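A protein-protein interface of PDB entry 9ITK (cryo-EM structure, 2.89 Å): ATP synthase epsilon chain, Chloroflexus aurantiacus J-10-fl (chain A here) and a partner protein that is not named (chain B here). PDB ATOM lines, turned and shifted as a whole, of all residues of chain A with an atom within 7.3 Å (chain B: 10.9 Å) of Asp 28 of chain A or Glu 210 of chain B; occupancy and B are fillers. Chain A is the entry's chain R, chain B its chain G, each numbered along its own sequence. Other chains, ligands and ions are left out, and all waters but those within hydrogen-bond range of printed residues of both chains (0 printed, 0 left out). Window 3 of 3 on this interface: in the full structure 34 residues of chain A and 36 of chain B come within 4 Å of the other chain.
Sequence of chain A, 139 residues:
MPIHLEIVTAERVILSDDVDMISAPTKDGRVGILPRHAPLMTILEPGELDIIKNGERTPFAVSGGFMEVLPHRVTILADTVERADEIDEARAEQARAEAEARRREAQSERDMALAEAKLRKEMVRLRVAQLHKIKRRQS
The backbone carbonyl oxygen of Met 41 of chain A is in hydrogen-bond range of the backbone NH of Glu 210 of chain B (3.3 Å). NZ of Lys 27 of chain A is in salt-bridge range of OE2 of Glu 215 of chain B (3.4 Å). OD2 of Asp 28 of chain A lies close to OE1 of Glu 210 of chain B, 2.9 Å away.
The backbone NH (N) of Lys 27 of chain A is in hydrogen-bond range of the backbone carbonyl oxygen (O) of Ile 43 of chain A (2.7 Å). N of Lys 27 of chain A sits at hydrogen-bond distance from OE1 of Glu 45 of chain A, 2.9 Å away.
Leu 40 of chain A touches Tyr 207 of chain B (O to CD2, 3.6 Å). Leu 40 of chain A touches Thr 208 of chain B (CD1 to OG1, 3.4 Å). Leu 40 of chain A touches Glu 210 of chain B (CD1 to CG, 3.6 Å). Tyr 207 of chain B touches Met 41 of chain A (CB to CB, 3.7 Å). Met 41 of chain A touches Thr 208 of chain B. Tyr 209 of chain B touches Met 41 of chain A. Val 216 of chain B touches Met 41 of chain A (CG1 to CE, 3.8 Å). Glu 210 of chain B touches Thr 42 of chain A (CB to CG2, 3.7 Å). CD1 of Ile 43 of chain A touches O of Glu 215 of chain B, 3.8 Å away. Ile 43 of chain A touches Val 216 of chain B.
No residue of chain B comes within 4 Å of Thr 26 of chain A. Asp 28 of chain A touches just one residue of chain B: Glu 210 (2.9 Å). No residue of chain B comes within 4 Å of Gly 29 of chain A. Of chain B, only Glu 210 comes within 4 Å of Thr 42 of chain A. Leu 56 of chain B touches none of the printed residues of chain A. Of the printed residues of chain A, Thr 208 of chain B touches Leu 40 and Met 41. Glu 210 of chain B touches four residues of chain A. Of the printed residues of chain A, Val 216 of chain B touches Met 41 (3.8 Å) and Ile 43 (3.6 Å). The nearest residue of chain A that does not touch Glu 210 of chain B is Thr 26 of chain A (4.2 Å).
Of the 13 printed residues of chain A, 6 touch a printed residue of chain B. Along chain A the printed residues that touch a printed residue of chain B span positions 27 to 43. Of the 13 printed residues of chain B, 7 touch a printed residue of chain A. Printed residues of chain B that touch a printed residue of chain A: Tyr 207, Thr 208, Tyr 209, Glu 210, Pro 211, Glu 215 and Val 216. Among the printed residues, 14 pairs touch across the chains.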
ATOM      1  N   PRO A  25      10.947   9.089  14.826  1.00  0.00           N
ATOM      2  CA  PRO A  25      10.097   9.333  16.010  1.00  0.00           C
ATOM      3  C   PRO A  25       8.655   8.860  15.819  1.00  0.00           C
ATOM      4  O   PRO A  25       7.741   9.620  15.512  1.00  0.00           O
ATOM      5  CB  PRO A  25      10.179  10.851  16.171  1.00  0.00           C
ATOM      6  CG  PRO A  25      10.345  11.355  14.778  1.00  0.00           C
ATOM      7  CD  PRO A  25      11.066  10.288  13.981  1.00  0.00           C
ATOM      8  N   THR A  26       8.450   7.558  15.982  1.00  0.00           N
ATOM      9  CA  THR A  26       7.119   6.977  15.873  1.00  0.00           C
ATOM     10  C   THR A  26       6.274   7.342  17.092  1.00  0.00           C
ATOM     11  O   THR A  26       6.794   7.607  18.177  1.00  0.00           O
ATOM     12  CB  THR A  26       7.226   5.459  15.716  1.00  0.00           C
ATOM     13  OG1 THR A  26       7.971   5.158  14.531  1.00  0.00           O
ATOM     14  CG2 THR A  26       5.865   4.806  15.614  1.00  0.00           C
ATOM     15  N   LYS A  27       4.951   7.365  16.893  1.00  0.00           N
ATOM     16  CA  LYS A  27       4.031   7.778  17.951  1.00  0.00           C
ATOM     17  C   LYS A  27       4.206   6.936  19.207  1.00  0.00           C
ATOM     18  O   LYS A  27       4.279   7.472  20.318  1.00  0.00           O
ATOM     19  CB  LYS A  27       2.590   7.699  17.453  1.00  0.00           C
ATOM     20  CG  LYS A  27       1.561   7.972  18.532  1.00  0.00           C
ATOM     21  CD  LYS A  27       0.151   8.009  17.972  1.00  0.00           C
ATOM     22  CE  LYS A  27      -0.088   9.270  17.161  1.00  0.00           C
ATOM     23  NZ  LYS A  27      -1.469   9.311  16.608  1.00  0.00           N
ATOM     24  N   ASP A  28       4.268   5.612  19.055  1.00  0.00           N
ATOM     25  CA  ASP A  28       4.464   4.767  20.228  1.00  0.00           C
ATOM     26  C   ASP A  28       5.826   5.019  20.860  1.00  0.00           C
ATOM     27  O   ASP A  28       5.950   5.046  22.090  1.00  0.00           O
ATOM     28  CB  ASP A  28       4.297   3.291  19.861  1.00  0.00           C
ATOM     29  CG  ASP A  28       5.386   2.791  18.937  1.00  0.00           C
ATOM     30  OD1 ASP A  28       6.523   2.575  19.407  1.00  0.00           O
ATOM     31  OD2 ASP A  28       5.102   2.606  17.739  1.00  0.00           O
ATOM     32  N   GLY A  29       6.851   5.211  20.043  1.00  0.00           N
ATOM     33  CA  GLY A  29       8.170   5.500  20.565  1.00  0.00           C
ATOM     34  C   GLY A  29       9.176   5.580  19.440  1.00  0.00           C
ATOM     35  O   GLY A  29       8.967   5.043  18.348  1.00  0.00           O
ATOM     36  N   ARG A  30      10.281   6.262  19.733  1.00  0.00           N
ATOM     37  CA  ARG A  30      11.333   6.442  18.743  1.00  0.00           C
ATOM     38  C   ARG A  30      11.891   5.095  18.306  1.00  0.00           C
ATOM     39  O   ARG A  30      12.190   4.235  19.139  1.00  0.00           O
ATOM     40  CB  ARG A  30      12.447   7.317  19.314  1.00  0.00           C
ATOM     41  CG  ARG A  30      13.703   7.345  18.469  1.00  0.00           C
ATOM     42  CD  ARG A  30      14.569   8.542  18.806  1.00  0.00           C
ATOM     43  NE  ARG A  30      13.821   9.792  18.767  1.00  0.00           N
ATOM     44  CZ  ARG A  30      13.704  10.557  17.692  1.00  0.00           C
ATOM     45  NH1 ARG A  30      14.261  10.220  16.541  1.00  0.00           N
ATOM     46  NH2 ARG A  30      13.011  11.689  17.774  1.00  0.00           N
ATOM     47  N   VAL A  31      12.033   4.915  16.997  1.00  0.00           N
ATOM     48  CA  VAL A  31      12.494   3.659  16.422  1.00  0.00           C
ATOM     49  C   VAL A  31      13.618   3.947  15.439  1.00  0.00           C
ATOM     50  O   VAL A  31      13.564   4.922  14.683  1.00  0.00           O
ATOM     51  CB  VAL A  31      11.340   2.893  15.733  1.00  0.00           C
ATOM     52  CG1 VAL A  31      10.741   3.719  14.617  1.00  0.00           C
ATOM     53  CG2 VAL A  31      11.823   1.557  15.196  1.00  0.00           C
ATOM     54  N   HIS A  37      15.325  -3.595   7.625  1.00  0.00           N
ATOM     55  CA  HIS A  37      14.255  -3.525   8.610  1.00  0.00           C
ATOM     56  C   HIS A  37      13.040  -4.323   8.152  1.00  0.00           C
ATOM     57  O   HIS A  37      12.737  -4.410   6.960  1.00  0.00           O
ATOM     58  CB  HIS A  37      13.862  -2.067   8.852  1.00  0.00           C
ATOM     59  CG  HIS A  37      13.142  -1.834  10.141  1.00  0.00           C
ATOM     60  ND1 HIS A  37      11.932  -2.422  10.437  1.00  0.00           N
ATOM     61  CD2 HIS A  37      13.453  -1.059  11.206  1.00  0.00           C
ATOM     62  CE1 HIS A  37      11.533  -2.028  11.633  1.00  0.00           C
ATOM     63  NE2 HIS A  37      12.437  -1.200  12.120  1.00  0.00           N
ATOM     64  N   LEU A  40       6.946  -2.461   8.020  1.00  0.00           N
ATOM     65  CA  LEU A  40       6.480  -1.590   9.085  1.00  0.00           C
ATOM     66  C   LEU A  40       5.651  -0.470   8.479  1.00  0.00           C
ATOM     67  O   LEU A  40       5.806  -0.136   7.302  1.00  0.00           O
ATOM     68  CB  LEU A  40       7.666  -1.027   9.872  1.00  0.00           C
ATOM     69  CG  LEU A  40       7.426  -0.222  11.143  1.00  0.00           C
ATOM     70  CD1 LEU A  40       7.318  -1.150  12.325  1.00  0.00           C
ATOM     71  CD2 LEU A  40       8.562   0.752  11.346  1.00  0.00           C
ATOM     72  N   MET A  41       4.767   0.100   9.291  1.00  0.00           N
ATOM     73  CA  MET A  41       3.955   1.238   8.870  1.00  0.00           C
ATOM     74  C   MET A  41       3.529   1.971  10.131  1.00  0.00           C
ATOM     75  O   MET A  41       2.744   1.439  10.919  1.00  0.00           O
ATOM     76  CB  MET A  41       2.747   0.787   8.057  1.00  0.00           C
ATOM     77  CG  MET A  41       1.705   1.868   7.856  1.00  0.00           C
ATOM     78  SD  MET A  41       2.312   3.215   6.827  1.00  0.00           S
ATOM     79  CE  MET A  41       1.013   4.424   7.043  1.00  0.00           C
ATOM     80  N   THR A  42       4.039   3.181  10.323  1.00  0.00           N
ATOM     81  CA  THR A  42       3.902   3.881  11.588  1.00  0.00           C
ATOM     82  C   THR A  42       3.246   5.236  11.385  1.00  0.00           C
ATOM     83  O   THR A  42       2.894   5.627  10.270  1.00  0.00           O
ATOM     84  CB  THR A  42       5.259   4.076  12.267  1.00  0.00           C
ATOM     85  OG1 THR A  42       6.108   4.857  11.420  1.00  0.00           O
ATOM     86  CG2 THR A  42       5.912   2.746  12.538  1.00  0.00           C
ATOM     87  N   ILE A  43       3.082   5.947  12.495  1.00  0.00           N
ATOM     88  CA  ILE A  43       2.590   7.317  12.512  1.00  0.00           C
ATOM     89  C   ILE A  43       3.605   8.168  13.256  1.00  0.00           C
ATOM     90  O   ILE A  43       4.031   7.809  14.359  1.00  0.00           O
ATOM     91  CB  ILE A  43       1.207   7.424  13.177  1.00  0.00           C
ATOM     92  CG1 ILE A  43       0.177   6.594  12.414  1.00  0.00           C
ATOM     93  CG2 ILE A  43       0.772   8.874  13.272  1.00  0.00           C
ATOM     94  CD1 ILE A  43      -1.000   6.176  13.259  1.00  0.00           C
ATOM     95  N   GLU A  45       4.875  11.891  15.008  1.00  0.00           N
ATOM     96  CA  GLU A  45       4.344  12.955  15.842  1.00  0.00           C
ATOM     97  C   GLU A  45       5.304  14.131  15.792  1.00  0.00           C
ATOM     98  O   GLU A  45       6.464  13.972  15.397  1.00  0.00           O
ATOM     99  CB  GLU A  45       4.154  12.489  17.294  1.00  0.00           C
ATOM    100  CG  GLU A  45       5.448  12.244  18.042  1.00  0.00           C
ATOM    101  CD  GLU A  45       5.989  10.860  17.802  1.00  0.00           C
ATOM    102  OE1 GLU A  45       5.525  10.216  16.841  1.00  0.00           O
ATOM    103  OE2 GLU A  45       6.874  10.420  18.564  1.00  0.00           O
ATOM    104  N   LEU B  56      -3.392  -1.579   2.786  1.00  0.00           N
ATOM    105  CA  LEU B  56      -4.030  -1.515   4.096  1.00  0.00           C
ATOM    106  C   LEU B  56      -5.489  -1.949   4.027  1.00  0.00           C
ATOM    107  O   LEU B  56      -5.942  -2.746   4.857  1.00  0.00           O
ATOM    108  CB  LEU B  56      -3.910  -0.104   4.668  1.00  0.00           C
ATOM    109  CG  LEU B  56      -4.138   0.080   6.170  1.00  0.00           C
ATOM    110  CD1 LEU B  56      -3.355   1.280   6.659  1.00  0.00           C
ATOM    111  CD2 LEU B  56      -5.608   0.238   6.507  1.00  0.00           C
ATOM    112  N   ASP B 206       2.203  -7.449   4.918  1.00  0.00           N
ATOM    113  CA  ASP B 206       1.601  -7.576   6.274  1.00  0.00           C
ATOM    114  C   ASP B 206       2.309  -6.577   7.191  1.00  0.00           C
ATOM    115  O   ASP B 206       2.979  -7.022   8.144  1.00  0.00           O
ATOM    116  CB  ASP B 206       1.677  -9.013   6.797  1.00  0.00           C
ATOM    117  CG  ASP B 206       0.877  -9.230   8.072  1.00  0.00           C
ATOM    118  OD1 ASP B 206       0.270  -8.254   8.557  1.00  0.00           O
ATOM    119  OD2 ASP B 206       0.864 -10.373   8.568  1.00  0.00           O
ATOM    120  N   TYR B 207       2.169  -5.279   6.909  1.00  0.00           N
ATOM    121  CA  TYR B 207       2.894  -4.246   7.694  1.00  0.00           C
ATOM    122  C   TYR B 207       2.555  -4.363   9.180  1.00  0.00           C
ATOM    123  O   TYR B 207       1.361  -4.419   9.516  1.00  0.00           O
ATOM    124  CB  TYR B 207       2.563  -2.843   7.177  1.00  0.00           C
ATOM    125  CG  TYR B 207       2.858  -2.632   5.713  1.00  0.00           C
ATOM    126  CD1 TYR B 207       1.834  -2.516   4.788  1.00  0.00           C
ATOM    127  CD2 TYR B 207       4.161  -2.560   5.250  1.00  0.00           C
ATOM    128  CE1 TYR B 207       2.096  -2.323   3.443  1.00  0.00           C
ATOM    129  CE2 TYR B 207       4.441  -2.370   3.907  1.00  0.00           C
ATOM    130  CZ  TYR B 207       3.404  -2.253   2.999  1.00  0.00           C
ATOM    131  OH  TYR B 207       3.666  -2.067   1.672  1.00  0.00           O
ATOM    132  N   THR B 208       3.575  -4.421  10.039  1.00  0.00           N
ATOM    133  CA  THR B 208       3.351  -4.435  11.480  1.00  0.00           C
ATOM    134  C   THR B 208       3.026  -3.007  11.908  1.00  0.00           C
ATOM    135  O   THR B 208       3.889  -2.243  12.337  1.00  0.00           O
ATOM    136  CB  THR B 208       4.567  -4.982  12.211  1.00  0.00           C
ATOM    137  OG1 THR B 208       5.651  -4.057  12.085  1.00  0.00           O
ATOM    138  CG2 THR B 208       4.984  -6.305  11.607  1.00  0.00           C
ATOM    139  N   TYR B 209       1.749  -2.651  11.783  1.00  0.00           N
ATOM    140  CA  TYR B 209       1.293  -1.305  12.101  1.00  0.00           C
ATOM    141  C   TYR B 209       1.561  -0.999  13.565  1.00  0.00           C
ATOM    142  O   TYR B 209       0.921  -1.576  14.450  1.00  0.00           O
ATOM    143  CB  TYR B 209      -0.195  -1.161  11.782  1.00  0.00           C
ATOM    144  CG  TYR B 209      -0.578  -1.729  10.436  1.00  0.00           C
ATOM    145  CD1 TYR B 209      -0.537  -0.946   9.293  1.00  0.00           C
ATOM    146  CD2 TYR B 209      -0.980  -3.050  10.309  1.00  0.00           C
ATOM    147  CE1 TYR B 209      -0.884  -1.464   8.063  1.00  0.00           C
ATOM    148  CE2 TYR B 209      -1.328  -3.576   9.084  1.00  0.00           C
ATOM    149  CZ  TYR B 209      -1.278  -2.779   7.965  1.00  0.00           C
ATOM    150  OH  TYR B 209      -1.625  -3.302   6.743  1.00  0.00           O
ATOM    151  N   GLU B 210       2.506  -0.090  13.835  1.00  0.00           N
ATOM    152  CA  GLU B 210       2.973   0.084  15.211  1.00  0.00           C
ATOM    153  C   GLU B 210       1.899   0.663  16.124  1.00  0.00           C
ATOM    154  O   GLU B 210       1.585   0.037  17.152  1.00  0.00           O
ATOM    155  CB  GLU B 210       4.260   0.911  15.227  1.00  0.00           C
ATOM    156  CG  GLU B 210       5.520   0.077  15.180  1.00  0.00           C
ATOM    157  CD  GLU B 210       5.743  -0.703  16.456  1.00  0.00           C
ATOM    158  OE1 GLU B 210       5.312  -0.230  17.525  1.00  0.00           O
ATOM    159  OE2 GLU B 210       6.351  -1.790  16.390  1.00  0.00           O
ATOM    160  N   PRO B 211       1.295   1.821  15.831  1.00  0.00           N
ATOM    161  CA  PRO B 211       0.276   2.350  16.750  1.00  0.00           C
ATOM    162  C   PRO B 211      -1.016   1.557  16.741  1.00  0.00           C
ATOM    163  O   PRO B 211      -1.900   1.844  17.558  1.00  0.00           O
ATOM    164  CB  PRO B 211       0.051   3.781  16.245  1.00  0.00           C
ATOM    165  CG  PRO B 211       1.191   4.056  15.315  1.00  0.00           C
ATOM    166  CD  PRO B 211       1.510   2.741  14.706  1.00  0.00           C
ATOM    167  N   GLY B 212      -1.155   0.577  15.854  1.00  0.00           N
ATOM    168  CA  GLY B 212      -2.372  -0.200  15.751  1.00  0.00           C
ATOM    169  C   GLY B 212      -2.966  -0.118  14.362  1.00  0.00           C
ATOM    170  O   GLY B 212      -2.918   0.941  13.730  1.00  0.00           O
ATOM    171  N   GLU B 213      -3.526  -1.225  13.871  1.00  0.00           N
ATOM    172  CA  GLU B 213      -4.093  -1.226  12.527  1.00  0.00           C
ATOM    173  C   GLU B 213      -5.236  -0.229  12.409  1.00  0.00           C
ATOM    174  O   GLU B 213      -5.340   0.493  11.411  1.00  0.00           O
ATOM    175  CB  GLU B 213      -4.571  -2.626  12.156  1.00  0.00           C
ATOM    176  CG  GLU B 213      -4.890  -2.788  10.684  1.00  0.00           C
ATOM    177  CD  GLU B 213      -4.623  -4.190  10.182  1.00  0.00           C
ATOM    178  OE1 GLU B 213      -3.970  -4.969  10.907  1.00  0.00           O
ATOM    179  OE2 GLU B 213      -5.071  -4.515   9.064  1.00  0.00           O
ATOM    180  N   GLU B 214      -6.108  -0.177  13.415  1.00  0.00           N
ATOM    181  CA  GLU B 214      -7.196   0.792  13.389  1.00  0.00           C
ATOM    182  C   GLU B 214      -6.674   2.211  13.563  1.00  0.00           C
ATOM    183  O   GLU B 214      -7.207   3.151  12.964  1.00  0.00           O
ATOM    184  CB  GLU B 214      -8.220   0.459  14.473  1.00  0.00           C
ATOM    185  CG  GLU B 214      -8.951  -0.852  14.240  1.00  0.00           C
ATOM    186  CD  GLU B 214      -9.845  -0.811  13.017  1.00  0.00           C
ATOM    187  OE1 GLU B 214     -10.378   0.273  12.702  1.00  0.00           O
ATOM    188  OE2 GLU B 214     -10.012  -1.865  12.367  1.00  0.00           O
ATOM    189  N   GLU B 215      -5.636   2.388  14.384  1.00  0.00           N
ATOM    190  CA  GLU B 215      -5.096   3.724  14.610  1.00  0.00           C
ATOM    191  C   GLU B 215      -4.497   4.307  13.337  1.00  0.00           C
ATOM    192  O   GLU B 215      -4.688   5.491  13.037  1.00  0.00           O
ATOM    193  CB  GLU B 215      -4.049   3.685  15.721  1.00  0.00           C
ATOM    194  CG  GLU B 215      -3.402   5.028  15.997  1.00  0.00           C
ATOM    195  CD  GLU B 215      -4.368   6.025  16.597  1.00  0.00           C
ATOM    196  OE1 GLU B 215      -5.327   5.593  17.271  1.00  0.00           O
ATOM    197  OE2 GLU B 215      -4.168   7.241  16.398  1.00  0.00           O
ATOM    198  N   VAL B 216      -3.759   3.494  12.580  1.00  0.00           N
ATOM    199  CA  VAL B 216      -3.174   3.971  11.332  1.00  0.00           C
ATOM    200  C   VAL B 216      -4.268   4.311  10.330  1.00  0.00           C
ATOM    201  O   VAL B 216      -4.239   5.366   9.687  1.00  0.00           O
ATOM    202  CB  VAL B 216      -2.196   2.927  10.766  1.00  0.00           C
ATOM    203  CG1 VAL B 216      -1.829   3.268   9.339  1.00  0.00           C
ATOM    204  CG2 VAL B 216      -0.955   2.845  11.629  1.00  0.00           C
ATOM    205  N   LEU B 217      -5.258   3.429  10.194  1.00  0.00           N
ATOM    206  CA  LEU B 217      -6.333   3.657   9.237  1.00  0.00           C
ATOM    207  C   LEU B 217      -7.137   4.902   9.588  1.00  0.00           C
ATOM    208  O   LEU B 217      -7.505   5.682   8.703  1.00  0.00           O
ATOM    209  CB  LEU B 217      -7.241   2.430   9.175  1.00  0.00           C
ATOM    210  CG  LEU B 217      -8.478   2.526   8.287  1.00  0.00           C
ATOM    211  CD1 LEU B 217      -8.076   2.796   6.852  1.00  0.00           C
ATOM    212  CD2 LEU B 217      -9.297   1.251   8.385  1.00  0.00           C
